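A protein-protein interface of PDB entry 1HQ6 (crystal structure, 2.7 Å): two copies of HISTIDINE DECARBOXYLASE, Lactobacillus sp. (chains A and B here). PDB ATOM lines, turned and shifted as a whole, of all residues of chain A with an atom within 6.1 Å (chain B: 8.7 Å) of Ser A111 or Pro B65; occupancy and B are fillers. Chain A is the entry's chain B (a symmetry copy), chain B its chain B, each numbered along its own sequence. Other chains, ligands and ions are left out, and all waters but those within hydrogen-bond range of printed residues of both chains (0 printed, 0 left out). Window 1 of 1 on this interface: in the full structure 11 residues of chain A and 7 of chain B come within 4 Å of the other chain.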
ATOM      1  C   PYR A   1       2.727  -7.908  -2.464  1.00  0.00           C
ATOM      2  O   PYR A   1       3.131  -7.192  -1.535  1.00  0.00           O
ATOM      3  CA  PYR A   1       2.235  -7.349  -3.647  1.00  0.00           C
ATOM      4  O3  PYR A   1       2.067  -6.120  -3.638  1.00  0.00           O
ATOM      5  CB  PYR A   1       1.979  -8.125  -4.929  1.00  0.00           C
ATOM      6  N   PHE A   2       2.841  -9.247  -2.403  1.00  0.00           N
ATOM      7  CA  PHE A   2       3.228  -9.907  -1.157  1.00  0.00           C
ATOM      8  C   PHE A   2       4.151 -11.103  -1.292  1.00  0.00           C
ATOM      9  O   PHE A   2       4.059 -11.840  -2.276  1.00  0.00           O
ATOM     10  CB  PHE A   2       2.029 -10.412  -0.416  1.00  0.00           C
ATOM     11  CG  PHE A   2       1.133  -9.312   0.070  1.00  0.00           C
ATOM     12  CD1 PHE A   2       1.522  -8.553   1.158  1.00  0.00           C
ATOM     13  CD2 PHE A   2      -0.064  -9.048  -0.579  1.00  0.00           C
ATOM     14  CE1 PHE A   2       0.710  -7.522   1.605  1.00  0.00           C
ATOM     15  CE2 PHE A   2      -0.872  -8.018  -0.132  1.00  0.00           C
ATOM     16  CZ  PHE A   2      -0.481  -7.257   0.956  1.00  0.00           C
ATOM     17  N   THR A   3       5.058 -11.325  -0.345  1.00  0.00           N
ATOM     18  CA  THR A   3       5.869 -12.533  -0.270  1.00  0.00           C
ATOM     19  C   THR A   3       5.611 -12.844   1.190  1.00  0.00           C
ATOM     20  O   THR A   3       5.661 -11.954   2.043  1.00  0.00           O
ATOM     21  CB  THR A   3       7.362 -12.299  -0.539  1.00  0.00           C
ATOM     22  OG1 THR A   3       7.939 -13.526  -0.153  1.00  0.00           O
ATOM     23  CG2 THR A   3       8.038 -11.170   0.192  1.00  0.00           C
ATOM     24  N   GLY A   4       5.261 -14.064   1.533  1.00  0.00           N
ATOM     25  CA  GLY A   4       4.810 -14.358   2.879  1.00  0.00           C
ATOM     26  C   GLY A   4       5.436 -15.589   3.465  1.00  0.00           C
ATOM     27  O   GLY A   4       6.647 -15.828   3.403  1.00  0.00           O
ATOM     28  N   VAL A   5       4.555 -16.422   3.985  1.00  0.00           N
ATOM     29  CA  VAL A   5       5.014 -17.640   4.635  1.00  0.00           C
ATOM     30  C   VAL A   5       5.834 -18.570   3.741  1.00  0.00           C
ATOM     31  O   VAL A   5       6.647 -19.311   4.255  1.00  0.00           O
ATOM     32  CB  VAL A   5       3.813 -18.418   5.219  1.00  0.00           C
ATOM     33  CG1 VAL A   5       3.228 -17.559   6.309  1.00  0.00           C
ATOM     34  CG2 VAL A   5       2.752 -18.732   4.193  1.00  0.00           C
ATOM     35  N   GLN A   6       5.742 -18.540   2.414  1.00  0.00           N
ATOM     36  CA  GLN A   6       6.475 -19.480   1.589  1.00  0.00           C
ATOM     37  C   GLN A   6       7.722 -18.876   0.986  1.00  0.00           C
ATOM     38  O   GLN A   6       8.310 -19.486   0.086  1.00  0.00           O
ATOM     39  CB  GLN A   6       5.612 -19.959   0.448  1.00  0.00           C
ATOM     40  CG  GLN A   6       4.326 -20.621   0.813  1.00  0.00           C
ATOM     41  CD  GLN A   6       3.293 -20.264  -0.219  1.00  0.00           C
ATOM     42  OE1 GLN A   6       2.971 -20.980  -1.167  1.00  0.00           O
ATOM     43  NE2 GLN A   6       2.732 -19.076  -0.066  1.00  0.00           N
ATOM     44  N   SER A 102       9.116  -4.601   2.241  1.00  0.00           N
ATOM     45  CA  SER A 102       9.071  -4.366   3.668  1.00  0.00           C
ATOM     46  C   SER A 102       8.909  -5.709   4.403  1.00  0.00           C
ATOM     47  O   SER A 102       7.960  -6.461   4.203  1.00  0.00           O
ATOM     48  CB  SER A 102       7.912  -3.388   3.892  1.00  0.00           C
ATOM     49  OG  SER A 102       7.953  -2.323   2.940  1.00  0.00           O
ATOM     50  N   PHE A 103       9.864  -6.063   5.256  1.00  0.00           N
ATOM     51  CA  PHE A 103       9.909  -7.328   5.965  1.00  0.00           C
ATOM     52  C   PHE A 103       9.022  -7.339   7.177  1.00  0.00           C
ATOM     53  O   PHE A 103       9.164  -6.473   8.036  1.00  0.00           O
ATOM     54  CB  PHE A 103      11.354  -7.592   6.348  1.00  0.00           C
ATOM     55  CG  PHE A 103      12.125  -7.843   5.072  1.00  0.00           C
ATOM     56  CD1 PHE A 103      11.821  -8.978   4.327  1.00  0.00           C
ATOM     57  CD2 PHE A 103      13.079  -6.945   4.601  1.00  0.00           C
ATOM     58  CE1 PHE A 103      12.454  -9.219   3.122  1.00  0.00           C
ATOM     59  CE2 PHE A 103      13.713  -7.183   3.391  1.00  0.00           C
ATOM     60  CZ  PHE A 103      13.399  -8.317   2.655  1.00  0.00           C
ATOM     61  N   ALA A 104       8.115  -8.301   7.287  1.00  0.00           N
ATOM     62  CA  ALA A 104       7.176  -8.350   8.393  1.00  0.00           C
ATOM     63  C   ALA A 104       7.855  -8.762   9.678  1.00  0.00           C
ATOM     64  O   ALA A 104       8.801  -9.551   9.680  1.00  0.00           O
ATOM     65  CB  ALA A 104       6.080  -9.337   8.118  1.00  0.00           C
ATOM     66  N   ASP A 106       6.510 -10.499  12.197  1.00  0.00           N
ATOM     67  CA  ASP A 106       6.261 -11.903  12.444  1.00  0.00           C
ATOM     68  C   ASP A 106       5.826 -12.619  11.179  1.00  0.00           C
ATOM     69  O   ASP A 106       4.618 -12.730  10.929  1.00  0.00           O
ATOM     70  CB  ASP A 106       5.182 -12.052  13.516  1.00  0.00           C
ATOM     71  CG  ASP A 106       4.962 -13.485  13.998  1.00  0.00           C
ATOM     72  OD1 ASP A 106       5.811 -14.352  13.738  1.00  0.00           O
ATOM     73  OD2 ASP A 106       3.939 -13.724  14.647  1.00  0.00           O
ATOM     74  N   PRO A 107       6.713 -13.211  10.378  1.00  0.00           N
ATOM     75  CA  PRO A 107       6.375 -13.856   9.116  1.00  0.00           C
ATOM     76  C   PRO A 107       5.581 -15.149   9.272  1.00  0.00           C
ATOM     77  O   PRO A 107       5.367 -15.879   8.316  1.00  0.00           O
ATOM     78  CB  PRO A 107       7.702 -14.064   8.455  1.00  0.00           C
ATOM     79  CG  PRO A 107       8.723 -13.306   9.276  1.00  0.00           C
ATOM     80  CD  PRO A 107       8.127 -13.367  10.665  1.00  0.00           C
ATOM     81  N   THR A 108       5.183 -15.533  10.476  1.00  0.00           N
ATOM     82  CA  THR A 108       4.356 -16.704  10.645  1.00  0.00           C
ATOM     83  C   THR A 108       2.890 -16.283  10.682  1.00  0.00           C
ATOM     84  O   THR A 108       1.970 -17.111  10.649  1.00  0.00           O
ATOM     85  CB  THR A 108       4.710 -17.376  11.942  1.00  0.00           C
ATOM     86  OG1 THR A 108       4.266 -16.460  12.929  1.00  0.00           O
ATOM     87  CG2 THR A 108       6.189 -17.614  12.150  1.00  0.00           C
ATOM     88  N   LYS A 109       2.681 -14.986  10.892  1.00  0.00           N
ATOM     89  CA  LYS A 109       1.339 -14.472  11.041  1.00  0.00           C
ATOM     90  C   LYS A 109       1.031 -13.467   9.963  1.00  0.00           C
ATOM     91  O   LYS A 109      -0.077 -13.465   9.436  1.00  0.00           O
ATOM     92  CB  LYS A 109       1.197 -13.816  12.396  1.00  0.00           C
ATOM     93  CG  LYS A 109      -0.174 -14.006  13.020  1.00  0.00           C
ATOM     94  CD  LYS A 109      -0.375 -13.148  14.277  1.00  0.00           C
ATOM     95  CE  LYS A 109      -1.734 -13.423  14.969  1.00  0.00           C
ATOM     96  NZ  LYS A 109      -2.890 -13.193  14.101  1.00  0.00           N
ATOM     97  N   ASP A 110       1.978 -12.605   9.617  1.00  0.00           N
ATOM     98  CA  ASP A 110       1.725 -11.562   8.644  1.00  0.00           C
ATOM     99  C   ASP A 110       2.683 -11.746   7.494  1.00  0.00           C
ATOM    100  O   ASP A 110       3.745 -12.360   7.667  1.00  0.00           O
ATOM    101  CB  ASP A 110       1.978 -10.165   9.192  1.00  0.00           C
ATOM    102  CG  ASP A 110       1.061  -9.678  10.299  1.00  0.00           C
ATOM    103  OD1 ASP A 110      -0.165  -9.813  10.175  1.00  0.00           O
ATOM    104  OD2 ASP A 110       1.591  -9.153  11.280  1.00  0.00           O
ATOM    105  N   SER A 111       2.346 -11.158   6.341  1.00  0.00           N
ATOM    106  CA  SER A 111       3.197 -11.212   5.166  1.00  0.00           C
ATOM    107  C   SER A 111       4.038  -9.978   5.032  1.00  0.00           C
ATOM    108  O   SER A 111       3.791  -8.945   5.656  1.00  0.00           O
ATOM    109  CB  SER A 111       2.355 -11.350   3.930  1.00  0.00           C
ATOM    110  OG  SER A 111       3.084 -11.422   2.711  1.00  0.00           O
ATOM    111  N   SER A 112       5.057 -10.132   4.211  1.00  0.00           N
ATOM    112  CA  SER A 112       5.930  -9.051   3.858  1.00  0.00           C
ATOM    113  C   SER A 112       5.365  -8.503   2.560  1.00  0.00           C
ATOM    114  O   SER A 112       4.803  -9.230   1.732  1.00  0.00           O
ATOM    115  CB  SER A 112       7.328  -9.620   3.711  1.00  0.00           C
ATOM    116  OG  SER A 112       7.738 -10.192   4.962  1.00  0.00           O
ATOM    117  N   MET A 113       5.521  -7.201   2.365  1.00  0.00           N
ATOM    118  CA  MET A 113       4.856  -6.487   1.286  1.00  0.00           C
ATOM    119  C   MET A 113       5.798  -5.792   0.328  1.00  0.00           C
ATOM    120  O   MET A 113       6.901  -5.396   0.700  1.00  0.00           O
ATOM    121  CB  MET A 113       3.911  -5.482   1.925  1.00  0.00           C
ATOM    122  CG  MET A 113       2.992  -4.630   1.051  1.00  0.00           C
ATOM    123  SD  MET A 113       2.120  -3.512   2.174  1.00  0.00           S
ATOM    124  CE  MET A 113       3.557  -2.503   2.451  1.00  0.00           C
ATOM    125  N   ALA A 153      -0.550  -5.189  10.258  1.00  0.00           N
ATOM    126  CA  ALA A 153       0.769  -5.737   9.989  1.00  0.00           C
ATOM    127  C   ALA A 153       1.808  -4.740  10.511  1.00  0.00           C
ATOM    128  O   ALA A 153       1.697  -3.521  10.294  1.00  0.00           O
ATOM    129  CB  ALA A 153       0.991  -5.925   8.487  1.00  0.00           C
ATOM    130  N   PHE A 155       5.966  -4.121  10.532  1.00  0.00           N
ATOM    131  CA  PHE A 155       7.172  -4.502   9.808  1.00  0.00           C
ATOM    132  C   PHE A 155       8.399  -4.122  10.629  1.00  0.00           C
ATOM    133  O   PHE A 155       8.264  -3.560  11.724  1.00  0.00           O
ATOM    134  CB  PHE A 155       7.243  -3.783   8.466  1.00  0.00           C
ATOM    135  CG  PHE A 155       6.078  -4.008   7.528  1.00  0.00           C
ATOM    136  CD1 PHE A 155       6.007  -5.141   6.742  1.00  0.00           C
ATOM    137  CD2 PHE A 155       5.063  -3.070   7.445  1.00  0.00           C
ATOM    138  CE1 PHE A 155       4.939  -5.334   5.880  1.00  0.00           C
ATOM    139  CE2 PHE A 155       3.989  -3.258   6.588  1.00  0.00           C
ATOM    140  CZ  PHE A 155       3.929  -4.393   5.804  1.00  0.00           C
ATOM    141  N   ARG B  59     -10.651 -13.398  12.407  1.00  0.00           N
ATOM    142  CA  ARG B  59     -10.146 -14.087  11.239  1.00  0.00           C
ATOM    143  C   ARG B  59     -10.334 -15.606  11.339  1.00  0.00           C
ATOM    144  O   ARG B  59      -9.933 -16.193  12.348  1.00  0.00           O
ATOM    145  CB  ARG B  59      -8.651 -13.758  11.063  1.00  0.00           C
ATOM    146  CG  ARG B  59      -8.300 -12.299  10.835  1.00  0.00           C
ATOM    147  CD  ARG B  59      -6.818 -12.112  10.553  1.00  0.00           C
ATOM    148  NE  ARG B  59      -6.452 -10.704  10.604  1.00  0.00           N
ATOM    149  CZ  ARG B  59      -5.247 -10.251  10.233  1.00  0.00           C
ATOM    150  NH1 ARG B  59      -4.967  -8.947  10.310  1.00  0.00           N
ATOM    151  NH2 ARG B  59      -4.304 -11.067   9.747  1.00  0.00           N
ATOM    152  N   TYR B  62      -8.938 -17.672   6.298  1.00  0.00           N
ATOM    153  CA  TYR B  62      -8.563 -16.688   5.304  1.00  0.00           C
ATOM    154  C   TYR B  62      -7.391 -17.215   4.535  1.00  0.00           C
ATOM    155  O   TYR B  62      -6.624 -18.019   5.057  1.00  0.00           O
ATOM    156  CB  TYR B  62      -8.189 -15.342   5.951  1.00  0.00           C
ATOM    157  CG  TYR B  62      -7.032 -15.327   6.929  1.00  0.00           C
ATOM    158  CD1 TYR B  62      -7.167 -15.891   8.188  1.00  0.00           C
ATOM    159  CD2 TYR B  62      -5.839 -14.713   6.568  1.00  0.00           C
ATOM    160  CE1 TYR B  62      -6.113 -15.830   9.101  1.00  0.00           C
ATOM    161  CE2 TYR B  62      -4.781 -14.649   7.471  1.00  0.00           C
ATOM    162  CZ  TYR B  62      -4.926 -15.207   8.743  1.00  0.00           C
ATOM    163  OH  TYR B  62      -3.901 -15.122   9.675  1.00  0.00           O
ATOM    164  N   PRO B  63      -7.192 -16.839   3.295  1.00  0.00           N
ATOM    165  CA  PRO B  63      -6.030 -17.234   2.531  1.00  0.00           C
ATOM    166  C   PRO B  63      -4.712 -16.809   3.154  1.00  0.00           C
ATOM    167  O   PRO B  63      -4.495 -15.702   3.642  1.00  0.00           O
ATOM    168  CB  PRO B  63      -6.312 -16.645   1.168  1.00  0.00           C
ATOM    169  CG  PRO B  63      -7.312 -15.558   1.415  1.00  0.00           C
ATOM    170  CD  PRO B  63      -8.188 -16.217   2.451  1.00  0.00           C
ATOM    171  N   ALA B  64      -3.817 -17.778   3.152  1.00  0.00           N
ATOM    172  CA  ALA B  64      -2.489 -17.661   3.712  1.00  0.00           C
ATOM    173  C   ALA B  64      -1.698 -16.440   3.332  1.00  0.00           C
ATOM    174  O   ALA B  64      -1.547 -16.177   2.150  1.00  0.00           O
ATOM    175  CB  ALA B  64      -1.647 -18.850   3.306  1.00  0.00           C
ATOM    176  N   PRO B  65      -1.117 -15.681   4.249  1.00  0.00           N
ATOM    177  CA  PRO B  65      -0.289 -14.541   3.937  1.00  0.00           C
ATOM    178  C   PRO B  65       0.806 -14.767   2.915  1.00  0.00           C
ATOM    179  O   PRO B  65       1.770 -15.497   3.143  1.00  0.00           O
ATOM    180  CB  PRO B  65       0.216 -14.125   5.293  1.00  0.00           C
ATOM    181  CG  PRO B  65      -0.059 -15.280   6.214  1.00  0.00           C
ATOM    182  CD  PRO B  65      -1.368 -15.772   5.672  1.00  0.00           C
ATOM    183  N   GLY B  66       0.673 -14.121   1.771  1.00  0.00           N
ATOM    184  CA  GLY B  66       1.653 -14.217   0.718  1.00  0.00           C
ATOM    185  C   GLY B  66       1.245 -15.200  -0.368  1.00  0.00           C
ATOM    186  O   GLY B  66       1.960 -15.353  -1.365  1.00  0.00           O
ATOM    187  N   SER B  67       0.115 -15.877  -0.233  1.00  0.00           N
ATOM    188  CA  SER B  67      -0.269 -16.833  -1.229  1.00  0.00           C
ATOM    189  C   SER B  67      -0.687 -16.196  -2.557  1.00  0.00           C
ATOM    190  O   SER B  67      -0.816 -14.975  -2.688  1.00  0.00           O
ATOM    191  CB  SER B  67      -1.380 -17.680  -0.624  1.00  0.00           C
ATOM    192  OG  SER B  67      -2.531 -16.953  -0.234  1.00  0.00           O
ATOM    193  N   PHE B  68      -0.838 -17.005  -3.586  1.00  0.00           N
ATOM    194  CA  PHE B  68      -1.257 -16.560  -4.879  1.00  0.00           C
ATOM    195  C   PHE B  68      -2.623 -17.139  -5.088  1.00  0.00           C
ATOM    196  O   PHE B  68      -2.776 -18.346  -5.224  1.00  0.00           O
ATOM    197  CB  PHE B  68      -0.297 -17.060  -5.927  1.00  0.00           C
ATOM    198  CG  PHE B  68       0.939 -16.202  -6.014  1.00  0.00           C
ATOM    199  CD1 PHE B  68       1.866 -16.171  -4.983  1.00  0.00           C
ATOM    200  CD2 PHE B  68       1.124 -15.418  -7.132  1.00  0.00           C
ATOM    201  CE1 PHE B  68       2.973 -15.353  -5.070  1.00  0.00           C
ATOM    202  CE2 PHE B  68       2.228 -14.601  -7.225  1.00  0.00           C
ATOM    203  CZ  PHE B  68       3.147 -14.572  -6.195  1.00  0.00           C
ATOM    204  N   ILE B  69      -3.642 -16.298  -5.078  1.00  0.00           N
ATOM    205  CA  ILE B  69      -5.021 -16.718  -5.234  1.00  0.00           C
ATOM    206  C   ILE B  69      -5.399 -16.140  -6.588  1.00  0.00           C
ATOM    207  O   ILE B  69      -5.222 -14.953  -6.874  1.00  0.00           O
ATOM    208  CB  ILE B  69      -5.901 -16.101  -4.145  1.00  0.00           C
ATOM    209  CG1 ILE B  69      -5.292 -16.273  -2.777  1.00  0.00           C
ATOM    210  CG2 ILE B  69      -7.275 -16.716  -4.247  1.00  0.00           C
ATOM    211  CD1 ILE B  69      -4.972 -17.685  -2.318  1.00  0.00           C
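No position is printed for both chains.
The side-chain hydroxyl (OG) of Ser B67 lies within hydrogen-bond range of the backbone carbonyl oxygen (O) of Ala B64 (2.7 Å).
OG of Ser A111 lies within hydrogen-bond range of O of Thr A3.
Hydrophobic or aromatic side chains of chain A that line the printed part of chain B: Phe A2 and Val A5.
Of the 9 printed residues of chain B, 3 touch a printed residue of chain A.
Printed residues of chain B that touch a printed residue of chain A: Pro B65, Gly B66 and Ser B67.
Hydrophobic or aromatic side chains of chain B within 4 Å of the printed part of chain A: Pro B65.
Among the printed residues, 8 pairs touch across the chains.
Among the printed residues, no Asp or Glu carboxylate lies within 4 Å of a Lys or Arg side-chain nitrogen of the other chain.
The backbone carbonyl oxygen (O) of Pro B65 lies within hydrogen-bond range of the backbone NH (N) of Val A5 (3.1 Å).
Among the printed residues, merely in contact across the chains: Phe A2 with Gly B66, Gly A4 with Pro B65, Gly A4 with Gly B66, Gln A6 with Ser B67, Lys A109 with Pro B65, Ser A111 with Pro B65 and Ser A111 with Gly B66.
Printed residues of chain B within 4 Å of Phe A2: Gly B66 (3.99 Å).
Of the printed residues of chain B, Gly A4 touches Pro B65 and Gly B66.
Of the printed residues of chain B, Gln A6 touches Ser B67 (3.9 Å).
Of the printed residues of chain B, Lys A109 touches Pro B65.
Ser A111 touches two residues of chain B.
No residue of chain B comes within 4 Å of Ser A112.
Ala A153 touches none of the printed residues of chain B.
Pro B65 touches four residues of chain A.
Ile B69 touches none of the printed residues of chain A.
The nearest residue of chain A that does not touch Pro B65 is Asp A110 (4.1 Å).
The nearest printed residue of chain B that does not touch Lys A109 is Tyr B62 (4.2 Å).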
